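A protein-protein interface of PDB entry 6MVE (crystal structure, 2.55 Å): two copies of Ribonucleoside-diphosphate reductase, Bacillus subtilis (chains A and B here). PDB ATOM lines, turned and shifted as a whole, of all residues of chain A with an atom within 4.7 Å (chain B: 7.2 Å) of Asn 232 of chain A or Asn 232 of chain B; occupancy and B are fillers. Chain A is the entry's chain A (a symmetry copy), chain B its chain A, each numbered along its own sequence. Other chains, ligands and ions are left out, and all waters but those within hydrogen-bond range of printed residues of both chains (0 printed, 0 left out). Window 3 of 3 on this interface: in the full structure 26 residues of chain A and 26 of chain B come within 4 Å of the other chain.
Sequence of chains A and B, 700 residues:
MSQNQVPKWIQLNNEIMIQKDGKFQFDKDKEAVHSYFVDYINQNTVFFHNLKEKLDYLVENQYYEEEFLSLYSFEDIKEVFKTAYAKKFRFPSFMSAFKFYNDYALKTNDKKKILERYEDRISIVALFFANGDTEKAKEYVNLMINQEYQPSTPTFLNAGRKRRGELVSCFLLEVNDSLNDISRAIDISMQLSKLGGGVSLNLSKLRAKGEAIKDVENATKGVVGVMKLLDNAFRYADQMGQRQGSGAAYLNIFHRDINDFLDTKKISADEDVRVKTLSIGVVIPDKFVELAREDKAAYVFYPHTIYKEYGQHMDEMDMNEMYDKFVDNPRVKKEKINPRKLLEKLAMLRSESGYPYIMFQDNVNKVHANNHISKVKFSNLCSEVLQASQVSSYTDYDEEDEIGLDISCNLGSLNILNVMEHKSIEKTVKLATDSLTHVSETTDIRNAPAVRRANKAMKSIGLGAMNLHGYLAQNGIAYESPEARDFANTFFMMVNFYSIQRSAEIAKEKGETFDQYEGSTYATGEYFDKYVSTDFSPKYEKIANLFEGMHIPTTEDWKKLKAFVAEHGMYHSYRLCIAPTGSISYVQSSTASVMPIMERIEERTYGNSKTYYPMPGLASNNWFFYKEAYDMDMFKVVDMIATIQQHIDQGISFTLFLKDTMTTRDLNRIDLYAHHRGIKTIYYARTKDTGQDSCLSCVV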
ATOM      1  N   LYS A 228      13.269   4.890  16.996  1.00  0.00           N
ATOM      2  CA  LYS A 228      14.265   4.364  17.927  1.00  0.00           C
ATOM      3  C   LYS A 228      14.917   3.107  17.366  1.00  0.00           C
ATOM      4  O   LYS A 228      16.144   2.967  17.406  1.00  0.00           O
ATOM      5  CB  LYS A 228      13.638   4.093  19.302  1.00  0.00           C
ATOM      6  N   LEU A 229      14.121   2.194  16.807  1.00  0.00           N
ATOM      7  CA  LEU A 229      14.715   0.995  16.225  1.00  0.00           C
ATOM      8  C   LEU A 229      15.598   1.342  15.027  1.00  0.00           C
ATOM      9  O   LEU A 229      16.688   0.782  14.872  1.00  0.00           O
ATOM     10  CB  LEU A 229      13.619  -0.004  15.833  1.00  0.00           C
ATOM     11  CG  LEU A 229      12.738  -0.600  16.932  1.00  0.00           C
ATOM     12  CD1 LEU A 229      11.521  -1.312  16.339  1.00  0.00           C
ATOM     13  CD2 LEU A 229      13.533  -1.542  17.816  1.00  0.00           C
ATOM     14  N   LEU A 230      15.148   2.262  14.164  1.00  0.00           N
ATOM     15  CA  LEU A 230      15.945   2.632  12.996  1.00  0.00           C
ATOM     16  C   LEU A 230      17.231   3.321  13.415  1.00  0.00           C
ATOM     17  O   LEU A 230      18.314   3.008  12.903  1.00  0.00           O
ATOM     18  CB  LEU A 230      15.142   3.536  12.073  1.00  0.00           C
ATOM     19  CG  LEU A 230      13.990   2.854  11.363  1.00  0.00           C
ATOM     20  CD1 LEU A 230      12.988   3.890  10.912  1.00  0.00           C
ATOM     21  CD2 LEU A 230      14.514   2.030  10.193  1.00  0.00           C
ATOM     22  N   ASP A 231      17.131   4.272  14.348  1.00  0.00           N
ATOM     23  CA  ASP A 231      18.328   4.921  14.857  1.00  0.00           C
ATOM     24  C   ASP A 231      19.355   3.886  15.249  1.00  0.00           C
ATOM     25  O   ASP A 231      20.537   4.012  14.918  1.00  0.00           O
ATOM     26  CB  ASP A 231      17.986   5.811  16.053  1.00  0.00           C
ATOM     27  CG  ASP A 231      19.199   6.554  16.585  1.00  0.00           C
ATOM     28  OD1 ASP A 231      19.824   7.311  15.809  1.00  0.00           O
ATOM     29  OD2 ASP A 231      19.537   6.380  17.773  1.00  0.00           O
ATOM     30  N   ASN A 232      18.906   2.815  15.900  1.00  0.00           N
ATOM     31  CA  ASN A 232      19.830   1.788  16.358  1.00  0.00           C
ATOM     32  C   ASN A 232      20.387   0.963  15.215  1.00  0.00           C
ATOM     33  O   ASN A 232      21.577   0.621  15.217  1.00  0.00           O
ATOM     34  CB  ASN A 232      19.140   0.886  17.352  1.00  0.00           C
ATOM     35  CG  ASN A 232      19.837   0.889  18.641  1.00  0.00           C
ATOM     36  OD1 ASN A 232      19.250   1.233  19.668  1.00  0.00           O
ATOM     37  ND2 ASN A 232      21.139   0.561  18.608  1.00  0.00           N
ATOM     38  N   ALA A 233      19.543   0.614  14.245  1.00  0.00           N
ATOM     39  CA  ALA A 233      20.027  -0.089  13.068  1.00  0.00           C
ATOM     40  C   ALA A 233      21.127   0.702  12.362  1.00  0.00           C
ATOM     41  O   ALA A 233      22.156   0.136  11.971  1.00  0.00           O
ATOM     42  CB  ALA A 233      18.859  -0.376  12.128  1.00  0.00           C
ATOM     43  N   PHE A 234      20.942   2.016  12.197  1.00  0.00           N
ATOM     44  CA  PHE A 234      21.962   2.805  11.514  1.00  0.00           C
ATOM     45  C   PHE A 234      23.239   2.907  12.345  1.00  0.00           C
ATOM     46  O   PHE A 234      24.341   2.921  11.793  1.00  0.00           O
ATOM     47  CB  PHE A 234      21.413   4.189  11.165  1.00  0.00           C
ATOM     48  CG  PHE A 234      20.428   4.174  10.040  1.00  0.00           C
ATOM     49  CD1 PHE A 234      20.832   3.855   8.762  1.00  0.00           C
ATOM     50  CD2 PHE A 234      19.104   4.488  10.253  1.00  0.00           C
ATOM     51  CE1 PHE A 234      19.927   3.826   7.718  1.00  0.00           C
ATOM     52  CE2 PHE A 234      18.188   4.463   9.213  1.00  0.00           C
ATOM     53  CZ  PHE A 234      18.600   4.133   7.947  1.00  0.00           C
ATOM     54  N   ARG A 235      23.109   2.966  13.670  1.00  0.00           N
ATOM     55  CA  ARG A 235      24.273   2.879  14.542  1.00  0.00           C
ATOM     56  C   ARG A 235      25.056   1.595  14.311  1.00  0.00           C
ATOM     57  O   ARG A 235      26.281   1.622  14.170  1.00  0.00           O
ATOM     58  CB  ARG A 235      23.836   2.933  15.995  1.00  0.00           C
ATOM     59  CG  ARG A 235      23.903   4.276  16.583  1.00  0.00           C
ATOM     60  CD  ARG A 235      23.594   4.194  18.047  1.00  0.00           C
ATOM     61  NE  ARG A 235      22.694   5.278  18.406  1.00  0.00           N
ATOM     62  CZ  ARG A 235      23.062   6.553  18.475  1.00  0.00           C
ATOM     63  NH1 ARG A 235      24.320   6.906  18.207  1.00  0.00           N
ATOM     64  NH2 ARG A 235      22.173   7.477  18.821  1.00  0.00           N
ATOM     65  N   TYR A 236      24.368   0.448  14.328  1.00  0.00           N
ATOM     66  CA  TYR A 236      25.064  -0.832  14.293  1.00  0.00           C
ATOM     67  C   TYR A 236      25.821  -1.016  12.976  1.00  0.00           C
ATOM     68  O   TYR A 236      27.005  -1.366  12.970  1.00  0.00           O
ATOM     69  CB  TYR A 236      24.069  -1.972  14.527  1.00  0.00           C
ATOM     70  CG  TYR A 236      24.715  -3.323  14.452  1.00  0.00           C
ATOM     71  CD1 TYR A 236      25.334  -3.871  15.551  1.00  0.00           C
ATOM     72  CD2 TYR A 236      24.713  -4.049  13.278  1.00  0.00           C
ATOM     73  CE1 TYR A 236      25.948  -5.098  15.485  1.00  0.00           C
ATOM     74  CE2 TYR A 236      25.310  -5.275  13.203  1.00  0.00           C
ATOM     75  CZ  TYR A 236      25.930  -5.798  14.304  1.00  0.00           C
ATOM     76  OH  TYR A 236      26.542  -7.029  14.236  1.00  0.00           O
ATOM     77  N   ILE B 186      16.298 -10.616  15.430  1.00  0.00           N
ATOM     78  CA  ILE B 186      15.564  -9.443  15.905  1.00  0.00           C
ATOM     79  C   ILE B 186      14.082  -9.582  15.600  1.00  0.00           C
ATOM     80  O   ILE B 186      13.231  -9.268  16.436  1.00  0.00           O
ATOM     81  CB  ILE B 186      16.117  -8.150  15.274  1.00  0.00           C
ATOM     82  CG1 ILE B 186      17.548  -7.876  15.711  1.00  0.00           C
ATOM     83  CG2 ILE B 186      15.232  -6.969  15.639  1.00  0.00           C
ATOM     84  CD1 ILE B 186      18.167  -6.733  14.901  1.00  0.00           C
ATOM     85  N   MET B 190      10.925 -10.350  18.285  1.00  0.00           N
ATOM     86  CA  MET B 190       9.761  -9.484  18.406  1.00  0.00           C
ATOM     87  C   MET B 190       8.471 -10.246  18.137  1.00  0.00           C
ATOM     88  O   MET B 190       7.438  -9.952  18.747  1.00  0.00           O
ATOM     89  CB  MET B 190       9.879  -8.283  17.461  1.00  0.00           C
ATOM     90  CG  MET B 190      10.886  -7.245  17.898  1.00  0.00           C
ATOM     91  SD  MET B 190      10.784  -5.650  17.056  1.00  0.00           S
ATOM     92  CE  MET B 190      10.963  -6.101  15.328  1.00  0.00           C
ATOM     93  N   GLY B 225      27.040  -5.137  20.463  1.00  0.00           N
ATOM     94  CA  GLY B 225      26.252  -4.439  19.461  1.00  0.00           C
ATOM     95  C   GLY B 225      24.936  -5.129  19.176  1.00  0.00           C
ATOM     96  O   GLY B 225      23.901  -4.477  19.014  1.00  0.00           O
ATOM     97  N   VAL B 226      24.952  -6.459  19.131  1.00  0.00           N
ATOM     98  CA  VAL B 226      23.729  -7.199  18.883  1.00  0.00           C
ATOM     99  C   VAL B 226      22.832  -7.202  20.117  1.00  0.00           C
ATOM    100  O   VAL B 226      21.604  -7.244  19.993  1.00  0.00           O
ATOM    101  CB  VAL B 226      24.079  -8.615  18.407  1.00  0.00           C
ATOM    102  CG1 VAL B 226      22.840  -9.433  18.236  1.00  0.00           C
ATOM    103  CG2 VAL B 226      24.835  -8.534  17.088  1.00  0.00           C
ATOM    104  N   MET B 227      23.404  -7.123  21.320  1.00  0.00           N
ATOM    105  CA  MET B 227      22.571  -6.985  22.512  1.00  0.00           C
ATOM    106  C   MET B 227      21.822  -5.660  22.516  1.00  0.00           C
ATOM    107  O   MET B 227      20.651  -5.607  22.920  1.00  0.00           O
ATOM    108  CB  MET B 227      23.420  -7.119  23.771  1.00  0.00           C
ATOM    109  CG  MET B 227      24.125  -8.447  23.876  1.00  0.00           C
ATOM    110  SD  MET B 227      25.256  -8.514  25.273  1.00  0.00           S
ATOM    111  CE  MET B 227      24.106  -8.466  26.654  1.00  0.00           C
ATOM    112  N   LYS B 228      22.477  -4.579  22.062  1.00  0.00           N
ATOM    113  CA  LYS B 228      21.800  -3.286  21.983  1.00  0.00           C
ATOM    114  C   LYS B 228      20.591  -3.364  21.062  1.00  0.00           C
ATOM    115  O   LYS B 228      19.508  -2.878  21.405  1.00  0.00           O
ATOM    116  CB  LYS B 228      22.772  -2.188  21.527  1.00  0.00           C
ATOM    117  N   LEU B 229      20.740  -4.001  19.899  1.00  0.00           N
ATOM    118  CA  LEU B 229      19.593  -4.129  19.006  1.00  0.00           C
ATOM    119  C   LEU B 229      18.496  -4.988  19.636  1.00  0.00           C
ATOM    120  O   LEU B 229      17.311  -4.658  19.536  1.00  0.00           O
ATOM    121  CB  LEU B 229      20.033  -4.702  17.654  1.00  0.00           C
ATOM    122  CG  LEU B 229      21.004  -3.892  16.792  1.00  0.00           C
ATOM    123  CD1 LEU B 229      21.569  -4.740  15.652  1.00  0.00           C
ATOM    124  CD2 LEU B 229      20.337  -2.641  16.250  1.00  0.00           C
ATOM    125  N   LEU B 230      18.869  -6.095  20.291  1.00  0.00           N
ATOM    126  CA  LEU B 230      17.865  -6.960  20.910  1.00  0.00           C
ATOM    127  C   LEU B 230      17.164  -6.245  22.051  1.00  0.00           C
ATOM    128  O   LEU B 230      15.933  -6.288  22.166  1.00  0.00           O
ATOM    129  CB  LEU B 230      18.510  -8.243  21.412  1.00  0.00           C
ATOM    130  CG  LEU B 230      18.986  -9.182  20.322  1.00  0.00           C
ATOM    131  CD1 LEU B 230      20.029 -10.120  20.881  1.00  0.00           C
ATOM    132  CD2 LEU B 230      17.802  -9.940  19.734  1.00  0.00           C
ATOM    133  N   ASP B 231      17.939  -5.579  22.913  1.00  0.00           N
ATOM    134  CA  ASP B 231      17.336  -4.805  23.986  1.00  0.00           C
ATOM    135  C   ASP B 231      16.249  -3.912  23.435  1.00  0.00           C
ATOM    136  O   ASP B 231      15.155  -3.829  23.998  1.00  0.00           O
ATOM    137  CB  ASP B 231      18.397  -3.971  24.705  1.00  0.00           C
ATOM    138  CG  ASP B 231      17.821  -3.185  25.870  1.00  0.00           C
ATOM    139  OD1 ASP B 231      17.251  -3.813  26.790  1.00  0.00           O
ATOM    140  OD2 ASP B 231      17.929  -1.943  25.870  1.00  0.00           O
ATOM    141  N   ASN B 232      16.513  -3.286  22.291  1.00  0.00           N
ATOM    142  CA  ASN B 232      15.544  -2.369  21.710  1.00  0.00           C
ATOM    143  C   ASN B 232      14.341  -3.091  21.135  1.00  0.00           C
ATOM    144  O   ASN B 232      13.205  -2.619  21.278  1.00  0.00           O
ATOM    145  CB  ASN B 232      16.203  -1.538  20.637  1.00  0.00           C
ATOM    146  CG  ASN B 232      16.104  -0.108  20.940  1.00  0.00           C
ATOM    147  OD1 ASN B 232      17.121   0.578  21.057  1.00  0.00           O
ATOM    148  ND2 ASN B 232      14.864   0.368  21.138  1.00  0.00           N
ATOM    149  N   ALA B 233      14.569  -4.219  20.464  1.00  0.00           N
ATOM    150  CA  ALA B 233      13.458  -5.018  19.972  1.00  0.00           C
ATOM    151  C   ALA B 233      12.519  -5.422  21.108  1.00  0.00           C
ATOM    152  O   ALA B 233      11.293  -5.331  20.972  1.00  0.00           O
ATOM    153  CB  ALA B 233      13.996  -6.241  19.234  1.00  0.00           C
ATOM    154  N   PHE B 234      13.069  -5.861  22.245  1.00  0.00           N
ATOM    155  CA  PHE B 234      12.207  -6.272  23.349  1.00  0.00           C
ATOM    156  C   PHE B 234      11.471  -5.080  23.954  1.00  0.00           C
ATOM    157  O   PHE B 234      10.320  -5.210  24.378  1.00  0.00           O
ATOM    158  CB  PHE B 234      13.022  -7.019  24.405  1.00  0.00           C
ATOM    159  CG  PHE B 234      13.427  -8.395  23.985  1.00  0.00           C
ATOM    160  CD1 PHE B 234      12.479  -9.380  23.813  1.00  0.00           C
ATOM    161  CD2 PHE B 234      14.751  -8.711  23.770  1.00  0.00           C
ATOM    162  CE1 PHE B 234      12.841 -10.652  23.413  1.00  0.00           C
ATOM    163  CE2 PHE B 234      15.124  -9.983  23.369  1.00  0.00           C
ATOM    164  CZ  PHE B 234      14.171 -10.953  23.191  1.00  0.00           C
ATOM    165  N   ARG B 235      12.112  -3.912  23.992  1.00  0.00           N
ATOM    166  CA  ARG B 235      11.421  -2.690  24.381  1.00  0.00           C
ATOM    167  C   ARG B 235      10.218  -2.414  23.492  1.00  0.00           C
ATOM    168  O   ARG B 235       9.125  -2.124  23.985  1.00  0.00           O
ATOM    169  CB  ARG B 235      12.373  -1.510  24.299  1.00  0.00           C
ATOM    170  CG  ARG B 235      13.007  -1.171  25.579  1.00  0.00           C
ATOM    171  CD  ARG B 235      13.807   0.086  25.421  1.00  0.00           C
ATOM    172  NE  ARG B 235      15.090  -0.078  26.083  1.00  0.00           N
ATOM    173  CZ  ARG B 235      15.244  -0.103  27.403  1.00  0.00           C
ATOM    174  NH1 ARG B 235      14.187   0.026  28.206  1.00  0.00           N
ATOM    175  NH2 ARG B 235      16.458  -0.248  27.921  1.00  0.00           N
ATOM    176  N   TYR B 236      10.416  -2.442  22.170  1.00  0.00           N
ATOM    177  CA  TYR B 236       9.363  -2.017  21.256  1.00  0.00           C
ATOM    178  C   TYR B 236       8.145  -2.938  21.345  1.00  0.00           C
ATOM    179  O   TYR B 236       7.008  -2.475  21.477  1.00  0.00           O
ATOM    180  CB  TYR B 236       9.909  -1.953  19.827  1.00  0.00           C
ATOM    181  CG  TYR B 236       8.860  -1.570  18.826  1.00  0.00           C
ATOM    182  CD1 TYR B 236       8.564  -0.248  18.587  1.00  0.00           C
ATOM    183  CD2 TYR B 236       8.158  -2.530  18.127  1.00  0.00           C
ATOM    184  CE1 TYR B 236       7.588   0.112  17.689  1.00  0.00           C
ATOM    185  CE2 TYR B 236       7.194  -2.185  17.223  1.00  0.00           C
ATOM    186  CZ  TYR B 236       6.906  -0.865  17.008  1.00  0.00           C
ATOM    187  OH  TYR B 236       5.930  -0.508  16.105  1.00  0.00           O
ATOM    188  N   ALA B 237       8.366  -4.250  21.309  1.00  0.00           N
ATOM    189  CA  ALA B 237       7.280  -5.218  21.170  1.00  0.00           C
ATOM    190  C   ALA B 237       6.790  -5.692  22.541  1.00  0.00           C
ATOM    191  O   ALA B 237       7.463  -6.486  23.202  1.00  0.00           O
ATOM    192  CB  ALA B 237       7.749  -6.404  20.327  1.00  0.00           C
ATOM    193  N   VAL B 275      22.412  -2.223  28.722  1.00  0.00           N
ATOM    194  CA  VAL B 275      21.315  -3.047  28.237  1.00  0.00           C
ATOM    195  C   VAL B 275      20.387  -3.246  29.419  1.00  0.00           C
ATOM    196  O   VAL B 275      20.842  -3.650  30.495  1.00  0.00           O
ATOM    197  CB  VAL B 275      21.831  -4.389  27.692  1.00  0.00           C
ATOM    198  CG1 VAL B 275      20.700  -5.322  27.505  1.00  0.00           C
ATOM    199  CG2 VAL B 275      22.577  -4.172  26.368  1.00  0.00           C
ATOM    200  N   THR B 277      16.696  -4.467  29.377  1.00  0.00           N
ATOM    201  CA  THR B 277      15.616  -5.442  29.456  1.00  0.00           C
ATOM    202  C   THR B 277      16.091  -6.874  29.258  1.00  0.00           C
ATOM    203  O   THR B 277      15.256  -7.780  29.171  1.00  0.00           O
ATOM    204  CB  THR B 277      14.514  -5.122  28.435  1.00  0.00           C
ATOM    205  OG1 THR B 277      14.815  -5.744  27.171  1.00  0.00           O
ATOM    206  CG2 THR B 277      14.380  -3.618  28.251  1.00  0.00           C
ATOM    207  N   LEU B 278      17.397  -7.106  29.164  1.00  0.00           N
ATOM    208  CA  LEU B 278      17.928  -8.424  28.841  1.00  0.00           C
ATOM    209  C   LEU B 278      18.519  -9.065  30.083  1.00  0.00           C
ATOM    210  O   LEU B 278      19.354  -8.460  30.753  1.00  0.00           O
ATOM    211  CB  LEU B 278      19.005  -8.353  27.754  1.00  0.00           C
ATOM    212  CG  LEU B 278      18.705  -8.053  26.289  1.00  0.00           C
ATOM    213  CD1 LEU B 278      20.011  -8.119  25.521  1.00  0.00           C
ATOM    214  CD2 LEU B 278      17.714  -9.027  25.709  1.00  0.00           C
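CD2 of Leu 229 of chain A touches O of Asn 232 of chain B, 3.6 Å away. Ala 233 of chain B touches Leu 229 of chain A. CG of Tyr 236 of chain B touches CD1 of Leu 229 of chain A, at 3.7 Å. Asn 232 of chain A touches Leu 229 of chain B. N of Ala 233 of chain A touches CD2 of Leu 229 of chain B, 3.9 Å away. Gly 225 of chain B touches Tyr 236 of chain A (O to CD1, 3.8 Å). Tyr 236 of chain A touches Val 226 of chain B. Tyr 236 of chain A touches Leu 229 of chain B.
Hydrophobic or aromatic side chains of chain B that line the printed part of chain A: Val 226, Leu 229 and Tyr 236. Among the printed residues, 9 pairs touch across the chains. Among the printed residues, no Asp or Glu carboxylate lies within 4 Å of a Lys or Arg side-chain nitrogen of the other chain.
Asn 232 of chain A touches just these residues of chain B: Leu 229 and Asn 232. Of chain A, only Leu 229 and Asn 232 come within 4 Å of Asn 232 of chain B. Of the printed residues of chain A, Val 226 of chain B touches Tyr 236 (3.6 Å). Of the printed residues of chain B, Leu 229 of chain A touches Asn 232, Ala 233 and Tyr 236. Of the printed residues of chain A, Tyr 236 of chain B touches Leu 229. Printed residues of chain A within 4 Å of Ala 233 of chain B: Leu 229. Of the printed residues of chain A, Gly 225 of chain B touches Tyr 236 (3.8 Å). Leu 230 of chain B touches none of the printed residues of chain A. Ile 186 of chain B touches none of the printed residues of chain A.
OD1 of Asn 232 of chain B lies close to OD1 of Asn 232 of chain A, at 2.6 Å.
Leu 229 of chain A touches Asn 232 of chain B, and with the chains exchanged Asn 232 of chain A touches Leu 229 of chain B. Leu 229 of chain A touches Ala 233 of chain B, and with the chains exchanged Ala 233 of chain A touches Leu 229 of chain B. Leu 229 of chain A touches Tyr 236 of chain B, and with the chains exchanged Tyr 236 of chain A touches Leu 229 of chain B. Asn 232 of chain B touches its own counterpart, Asn 232 of chain A. Positions printed for both chains: 228, 229, 230, 231, 232, 233, 234, 235 and 236.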
